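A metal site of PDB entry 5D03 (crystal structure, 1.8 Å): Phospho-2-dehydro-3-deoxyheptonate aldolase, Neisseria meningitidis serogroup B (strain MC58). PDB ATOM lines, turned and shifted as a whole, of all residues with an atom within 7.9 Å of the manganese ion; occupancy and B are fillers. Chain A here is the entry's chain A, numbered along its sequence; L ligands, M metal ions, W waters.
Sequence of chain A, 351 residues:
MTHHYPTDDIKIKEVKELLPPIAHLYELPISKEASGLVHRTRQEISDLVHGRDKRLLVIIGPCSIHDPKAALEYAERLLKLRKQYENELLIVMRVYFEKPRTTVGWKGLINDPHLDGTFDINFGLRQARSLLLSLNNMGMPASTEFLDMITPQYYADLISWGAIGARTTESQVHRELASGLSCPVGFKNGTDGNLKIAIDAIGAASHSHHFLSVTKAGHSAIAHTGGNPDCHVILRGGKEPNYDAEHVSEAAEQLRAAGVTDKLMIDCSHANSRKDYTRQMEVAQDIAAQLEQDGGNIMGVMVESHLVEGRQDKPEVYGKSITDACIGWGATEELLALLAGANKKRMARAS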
ATOM      1  N   GLY A  61     -18.522  -5.200 -14.802  1.00  0.00           N
ATOM      2  CA  GLY A  61     -19.197  -5.023 -13.507  1.00  0.00           C
ATOM      3  C   GLY A  61     -18.369  -5.538 -12.355  1.00  0.00           C
ATOM      4  O   GLY A  61     -17.187  -5.738 -12.515  1.00  0.00           O
ATOM      5  N   PRO A  62     -18.982  -5.724 -11.186  1.00  0.00           N
ATOM      6  CA  PRO A  62     -18.235  -6.029  -9.967  1.00  0.00           C
ATOM      7  C   PRO A  62     -17.433  -7.325 -10.041  1.00  0.00           C
ATOM      8  O   PRO A  62     -17.771  -8.243 -10.799  1.00  0.00           O
ATOM      9  CB  PRO A  62     -19.334  -6.175  -8.923  1.00  0.00           C
ATOM     10  CG  PRO A  62     -20.457  -5.287  -9.443  1.00  0.00           C
ATOM     11  CD  PRO A  62     -20.421  -5.444 -10.932  1.00  0.00           C
ATOM     12  N   CYS A  63     -16.323  -7.366  -9.313  1.00  0.00           N
ATOM     13  CA  CYS A  63     -15.595  -8.598  -9.174  1.00  0.00           C
ATOM     14  C   CYS A  63     -16.520  -9.665  -8.608  1.00  0.00           C
ATOM     15  O   CYS A  63     -16.589 -10.809  -9.090  1.00  0.00           O
ATOM     16  CB  CYS A  63     -14.385  -8.367  -8.249  1.00  0.00           C
ATOM     17  SG  CYS A  63     -13.518  -9.929  -7.795  1.00  0.00           S
ATOM     18  N   SER A  64     -17.255  -9.308  -7.570  1.00  0.00           N
ATOM     19  CA  SER A  64     -18.248 -10.169  -7.004  1.00  0.00           C
ATOM     20  C   SER A  64     -19.511  -9.413  -6.600  1.00  0.00           C
ATOM     21  O   SER A  64     -19.467  -8.216  -6.256  1.00  0.00           O
ATOM     22  CB  SER A  64     -17.682 -10.840  -5.750  1.00  0.00           C
ATOM     23  OG  SER A  64     -17.332  -9.886  -4.733  1.00  0.00           O
ATOM     24  N   ARG A  94     -21.273  -8.188 -15.374  1.00  0.00           N
ATOM     25  CA  ARG A  94     -20.649  -9.195 -14.519  1.00  0.00           C
ATOM     26  C   ARG A  94     -21.555  -9.378 -13.337  1.00  0.00           C
ATOM     27  O   ARG A  94     -21.755  -8.450 -12.550  1.00  0.00           O
ATOM     28  CB  ARG A  94     -19.262  -8.776 -13.988  1.00  0.00           C
ATOM     29  CG  ARG A  94     -18.126  -8.950 -14.941  1.00  0.00           C
ATOM     30  CD  ARG A  94     -16.755  -8.596 -14.351  1.00  0.00           C
ATOM     31  NE  ARG A  94     -16.469  -9.331 -13.132  1.00  0.00           N
ATOM     32  CZ  ARG A  94     -15.517 -10.249 -12.981  1.00  0.00           C
ATOM     33  NH1 ARG A  94     -14.700 -10.601 -13.972  1.00  0.00           N
ATOM     34  NH2 ARG A  94     -15.406 -10.841 -11.829  1.00  0.00           N
ATOM     35  N   TYR A  96     -21.184 -12.086 -10.733  1.00  0.00           N
ATOM     36  CA  TYR A  96     -20.433 -13.254 -10.243  1.00  0.00           C
ATOM     37  C   TYR A  96     -20.806 -13.676  -8.843  1.00  0.00           C
ATOM     38  O   TYR A  96     -20.688 -12.907  -7.869  1.00  0.00           O
ATOM     39  CB  TYR A  96     -18.962 -12.958 -10.342  1.00  0.00           C
ATOM     40  CG  TYR A  96     -18.320 -13.095 -11.722  1.00  0.00           C
ATOM     41  CD1 TYR A  96     -18.920 -12.598 -12.881  1.00  0.00           C
ATOM     42  CD2 TYR A  96     -17.136 -13.749 -11.875  1.00  0.00           C
ATOM     43  CE1 TYR A  96     -18.326 -12.724 -14.134  1.00  0.00           C
ATOM     44  CE2 TYR A  96     -16.528 -13.856 -13.124  1.00  0.00           C
ATOM     45  CZ  TYR A  96     -17.129 -13.319 -14.251  1.00  0.00           C
ATOM     46  OH  TYR A  96     -16.583 -13.425 -15.509  1.00  0.00           O
ATOM     47  N   LYS A  99     -16.701 -17.373  -6.207  1.00  0.00           N
ATOM     48  CA  LYS A  99     -15.329 -16.884  -6.257  1.00  0.00           C
ATOM     49  C   LYS A  99     -14.333 -17.944  -5.853  1.00  0.00           C
ATOM     50  O   LYS A  99     -14.457 -18.558  -4.766  1.00  0.00           O
ATOM     51  CB  LYS A  99     -15.197 -15.699  -5.288  1.00  0.00           C
ATOM     52  CG  LYS A  99     -16.187 -14.580  -5.526  1.00  0.00           C
ATOM     53  CD  LYS A  99     -16.153 -14.012  -6.956  1.00  0.00           C
ATOM     54  CE  LYS A  99     -14.838 -13.391  -7.396  1.00  0.00           C
ATOM     55  NZ  LYS A  99     -14.805 -13.012  -8.817  1.00  0.00           N
ATOM     56  N   PRO A 100     -13.292 -18.132  -6.691  1.00  0.00           N
ATOM     57  CA  PRO A 100     -12.237 -19.105  -6.398  1.00  0.00           C
ATOM     58  C   PRO A 100     -11.204 -18.429  -5.545  1.00  0.00           C
ATOM     59  O   PRO A 100     -10.707 -17.383  -5.925  1.00  0.00           O
ATOM     60  CB  PRO A 100     -11.695 -19.464  -7.778  1.00  0.00           C
ATOM     61  CG  PRO A 100     -11.971 -18.308  -8.668  1.00  0.00           C
ATOM     62  CD  PRO A 100     -13.232 -17.644  -8.108  1.00  0.00           C
ATOM     63  N   GLU A 145     -19.092 -16.558 -13.482  1.00  0.00           N
ATOM     64  CA  GLU A 145     -18.150 -17.649 -13.530  1.00  0.00           C
ATOM     65  C   GLU A 145     -18.852 -18.865 -12.973  1.00  0.00           C
ATOM     66  O   GLU A 145     -19.398 -18.818 -11.855  1.00  0.00           O
ATOM     67  CB  GLU A 145     -16.844 -17.395 -12.690  1.00  0.00           C
ATOM     68  CG  GLU A 145     -15.966 -18.646 -12.700  1.00  0.00           C
ATOM     69  CD  GLU A 145     -14.678 -18.612 -11.863  1.00  0.00           C
ATOM     70  OE1 GLU A 145     -14.192 -17.504 -11.551  1.00  0.00           O
ATOM     71  OE2 GLU A 145     -14.157 -19.731 -11.575  1.00  0.00           O
ATOM     72  N   ARG A 167      -8.200 -20.839 -12.699  1.00  0.00           N
ATOM     73  CA  ARG A 167      -7.793 -21.923 -11.777  1.00  0.00           C
ATOM     74  C   ARG A 167      -8.477 -23.269 -12.126  1.00  0.00           C
ATOM     75  O   ARG A 167      -8.183 -24.267 -11.510  1.00  0.00           O
ATOM     76  CB  ARG A 167      -8.106 -21.543 -10.360  1.00  0.00           C
ATOM     77  CG  ARG A 167      -7.219 -20.387  -9.916  1.00  0.00           C
ATOM     78  CD  ARG A 167      -7.590 -19.796  -8.566  1.00  0.00           C
ATOM     79  NE  ARG A 167      -6.798 -18.581  -8.332  1.00  0.00           N
ATOM     80  CZ  ARG A 167      -7.057 -17.386  -8.885  1.00  0.00           C
ATOM     81  NH1 ARG A 167      -8.113 -17.184  -9.693  1.00  0.00           N
ATOM     82  NH2 ARG A 167      -6.269 -16.350  -8.626  1.00  0.00           N
ATOM     83  N   LYS A 188     -10.406 -18.822 -19.364  1.00  0.00           N
ATOM     84  CA  LYS A 188      -9.254 -17.992 -19.052  1.00  0.00           C
ATOM     85  C   LYS A 188      -7.966 -18.771 -19.144  1.00  0.00           C
ATOM     86  O   LYS A 188      -7.933 -19.932 -18.824  1.00  0.00           O
ATOM     87  CB  LYS A 188      -9.417 -17.447 -17.684  1.00  0.00           C
ATOM     88  CG  LYS A 188     -10.487 -16.386 -17.696  1.00  0.00           C
ATOM     89  CD  LYS A 188     -10.561 -15.684 -16.414  1.00  0.00           C
ATOM     90  CE  LYS A 188     -10.812 -14.222 -16.700  1.00  0.00           C
ATOM     91  NZ  LYS A 188     -10.685 -13.457 -15.438  1.00  0.00           N
ATOM     92  N   ASP A 267      -9.108  -9.598 -20.824  1.00  0.00           N
ATOM     93  CA  ASP A 267      -9.449  -9.140 -19.485  1.00  0.00           C
ATOM     94  C   ASP A 267      -8.523  -7.953 -19.165  1.00  0.00           C
ATOM     95  O   ASP A 267      -7.317  -8.120 -19.148  1.00  0.00           O
ATOM     96  CB  ASP A 267      -9.313 -10.315 -18.471  1.00  0.00           C
ATOM     97  CG  ASP A 267      -9.738  -9.926 -17.000  1.00  0.00           C
ATOM     98  OD1 ASP A 267     -10.148  -8.770 -16.739  1.00  0.00           O
ATOM     99  OD2 ASP A 267      -9.664 -10.811 -16.130  1.00  0.00           O
ATOM    100  N   SER A 269      -8.376  -6.650 -16.191  1.00  0.00           N
ATOM    101  CA  SER A 269      -8.091  -6.732 -14.749  1.00  0.00           C
ATOM    102  C   SER A 269      -7.170  -7.924 -14.448  1.00  0.00           C
ATOM    103  O   SER A 269      -6.356  -8.355 -15.317  1.00  0.00           O
ATOM    104  CB  SER A 269      -9.419  -6.860 -13.996  1.00  0.00           C
ATOM    105  OG  SER A 269      -9.318  -6.413 -12.665  1.00  0.00           O
ATOM    106  N   HIS A 270      -7.296  -8.420 -13.220  1.00  0.00           N
ATOM    107  CA  HIS A 270      -6.499  -9.531 -12.701  1.00  0.00           C
ATOM    108  C   HIS A 270      -5.047  -9.381 -13.054  1.00  0.00           C
ATOM    109  O   HIS A 270      -4.463  -8.343 -12.759  1.00  0.00           O
ATOM    110  CB  HIS A 270      -7.151 -10.833 -13.135  1.00  0.00           C
ATOM    111  CG  HIS A 270      -8.562 -10.869 -12.693  1.00  0.00           C
ATOM    112  ND1 HIS A 270      -9.623 -10.617 -13.542  1.00  0.00           N
ATOM    113  CD2 HIS A 270      -9.100 -11.001 -11.445  1.00  0.00           C
ATOM    114  CE1 HIS A 270     -10.744 -10.605 -12.844  1.00  0.00           C
ATOM    115  NE2 HIS A 270     -10.456 -10.845 -11.574  1.00  0.00           N
ATOM    116  N   MET A 302     -13.138  -7.659 -20.866  1.00  0.00           N
ATOM    117  CA  MET A 302     -13.648  -7.823 -19.530  1.00  0.00           C
ATOM    118  C   MET A 302     -13.077  -6.746 -18.630  1.00  0.00           C
ATOM    119  O   MET A 302     -11.897  -6.422 -18.716  1.00  0.00           O
ATOM    120  CB  MET A 302     -13.319  -9.233 -18.992  1.00  0.00           C
ATOM    121  CG  MET A 302     -13.763  -9.477 -17.571  1.00  0.00           C
ATOM    122  SD  MET A 302     -13.324 -11.195 -16.957  1.00  0.00           S
ATOM    123  CE  MET A 302     -14.146 -12.166 -18.205  1.00  0.00           C
ATOM    124  N   GLU A 304     -13.483  -5.008 -14.430  1.00  0.00           N
ATOM    125  CA  GLU A 304     -13.928  -5.034 -13.068  1.00  0.00           C
ATOM    126  C   GLU A 304     -14.265  -3.632 -12.613  1.00  0.00           C
ATOM    127  O   GLU A 304     -13.395  -2.808 -12.422  1.00  0.00           O
ATOM    128  CB  GLU A 304     -12.875  -5.703 -12.187  1.00  0.00           C
ATOM    129  CG  GLU A 304     -12.949  -7.223 -12.368  1.00  0.00           C
ATOM    130  CD  GLU A 304     -12.151  -7.992 -11.340  1.00  0.00           C
ATOM    131  OE1 GLU A 304     -10.973  -7.668 -11.057  1.00  0.00           O
ATOM    132  OE2 GLU A 304     -12.719  -8.948 -10.833  1.00  0.00           O
ATOM    133  N   SER A 321     -16.438  -2.933  -3.735  1.00  0.00           N
ATOM    134  CA  SER A 321     -16.058  -4.368  -3.737  1.00  0.00           C
ATOM    135  C   SER A 321     -15.467  -4.838  -2.409  1.00  0.00           C
ATOM    136  O   SER A 321     -14.714  -4.111  -1.798  1.00  0.00           O
ATOM    137  CB  SER A 321     -14.999  -4.612  -4.827  1.00  0.00           C
ATOM    138  OG  SER A 321     -14.655  -6.010  -4.979  1.00  0.00           O
ATOM    139  N   THR A 323     -14.032  -7.968  -2.733  1.00  0.00           N
ATOM    140  CA  THR A 323     -13.027  -8.861  -3.295  1.00  0.00           C
ATOM    141  C   THR A 323     -12.009  -7.979  -4.046  1.00  0.00           C
ATOM    142  O   THR A 323     -11.499  -7.028  -3.462  1.00  0.00           O
ATOM    143  CB  THR A 323     -13.703  -9.988  -4.116  1.00  0.00           C
ATOM    144  OG1 THR A 323     -14.686  -9.484  -5.025  1.00  0.00           O
ATOM    145  CG2 THR A 323     -14.407 -10.939  -3.175  1.00  0.00           C
ATOM    146  N   ASP A 324     -11.751  -8.226  -5.332  1.00  0.00           N
ATOM    147  CA  ASP A 324     -10.757  -7.432  -6.052  1.00  0.00           C
ATOM    148  C   ASP A 324     -11.215  -5.977  -6.170  1.00  0.00           C
ATOM    149  O   ASP A 324     -12.421  -5.673  -6.320  1.00  0.00           O
ATOM    150  CB  ASP A 324     -10.523  -7.986  -7.472  1.00  0.00           C
ATOM    151  CG  ASP A 324      -9.930  -9.382  -7.461  1.00  0.00           C
ATOM    152  OD1 ASP A 324      -9.235  -9.732  -6.515  1.00  0.00           O
ATOM    153  OD2 ASP A 324     -10.163 -10.142  -8.396  1.00  0.00           O
ATOM    154  N   ALA A 325     -10.246  -5.068  -6.157  1.00  0.00           N
ATOM    155  CA  ALA A 325     -10.555  -3.660  -6.389  1.00  0.00           C
ATOM    156  C   ALA A 325     -11.073  -3.412  -7.818  1.00  0.00           C
ATOM    157  O   ALA A 325     -10.579  -4.017  -8.761  1.00  0.00           O
ATOM    158  CB  ALA A 325      -9.364  -2.756  -6.033  1.00  0.00           C
ATOM    159  N   CYS A 326     -12.068  -2.536  -7.939  1.00  0.00           N
ATOM    160  CA  CYS A 326     -12.722  -2.198  -9.177  1.00  0.00           C
ATOM    161  C   CYS A 326     -12.564  -0.695  -9.478  1.00  0.00           C
ATOM    162  O   CYS A 326     -12.422   0.130  -8.550  1.00  0.00           O
ATOM    163  CB  CYS A 326     -14.214  -2.509  -9.059  1.00  0.00           C
ATOM    164  SG  CYS A 326     -14.597  -4.251  -8.811  1.00  0.00           S
HETATM  165  C1  LIG L   1     -12.732 -13.191 -12.100  1.00  0.00           C
HETATM  166  O1  LIG L   1     -12.884 -12.869 -13.317  1.00  0.00           O
HETATM  167  O2  LIG L   1     -13.247 -12.600 -11.139  1.00  0.00           O
HETATM  168  C2  LIG L   1     -11.774 -14.226 -11.766  1.00  0.00           C
HETATM  169  C3  LIG L   1     -11.912 -14.999 -10.688  1.00  0.00           C
HETATM  170  O3  LIG L   1     -10.639 -14.192 -12.633  1.00  0.00           O
HETATM  171  P1  LIG L   1      -9.407 -15.297 -12.787  1.00  0.00           P
HETATM  172  O4  LIG L   1     -10.061 -16.668 -12.933  1.00  0.00           O
HETATM  173  O5  LIG L   1      -8.764 -14.699 -14.016  1.00  0.00           O
HETATM  174  O6  LIG L   1      -8.615 -15.126 -11.528  1.00  0.00           O
HETATM  175 MN    MN M   1     -11.820 -10.472  -9.676  1.00  0.00          MN
HETATM  176  O   HOH W   1     -11.911 -12.372  -8.823  1.00  0.00           O
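An oxygen (O6) of the ligand lies within salt-bridge range of the guanidinium group of Arg 167 (2.8 Å). The guanidinium group (NH2) of Arg 94 lies within salt-bridge range of an oxygen (O2) of the ligand. An oxygen (O2) of the ligand is in salt-bridge range of the side-chain amino group of Lys 99 (2.8 Å). A ring nitrogen (NE2) of His 270 sits close to an oxygen (O2) of the ligand, 3.3 Å away. NZ of Lys 188 is in salt-bridge range of O5 of the ligand (2.7 Å).
The side-chain carboxylate of Glu 304 is in hydrogen-bond range of the side-chain hydroxyl of Ser 269 (2.6 Å). OE2 of Glu 304 sits close to NH2 of Arg 94, 3.4 Å away. The backbone carbonyl oxygen (O) of Cys 63 sits at hydrogen-bond distance from the side-chain amino group (NZ) of Lys 99. The backbone carbonyl oxygen (O) of Asp 324 lies within hydrogen-bond range of the side-chain hydroxyl (OG) of Ser 321 (2.6 Å). The guanidinium group (NH2) of Arg 94 is in hydrogen-bond range of the backbone carbonyl oxygen (O) of Cys 63 (3.0 Å). N of Cys 63 is in hydrogen-bond range of SG of Cys 326 (3.6 Å). O of Asp 324 sits at hydrogen-bond distance from SG of Cys 326. OD2 of Asp 267 lies within hydrogen-bond range of ND1 of His 270, 2.6 Å away.
Within 4 Å of the manganese ion: Cys 63, His 270, Glu 304 and Asp 324. Along chain A the residues within 4 Å of the manganese ion span positions 63 to 324.
The manganese ion is bound by water W1, OE2 of Glu 304, OD2 of Asp 324, NE2 of His 270 and SG of Cys 63. The manganese ion has five donor atoms within binding distance.
Water W1 lies within hydrogen-bond range of an oxygen (O2) of the ligand and the side-chain amino group (NZ) of Lys 99.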
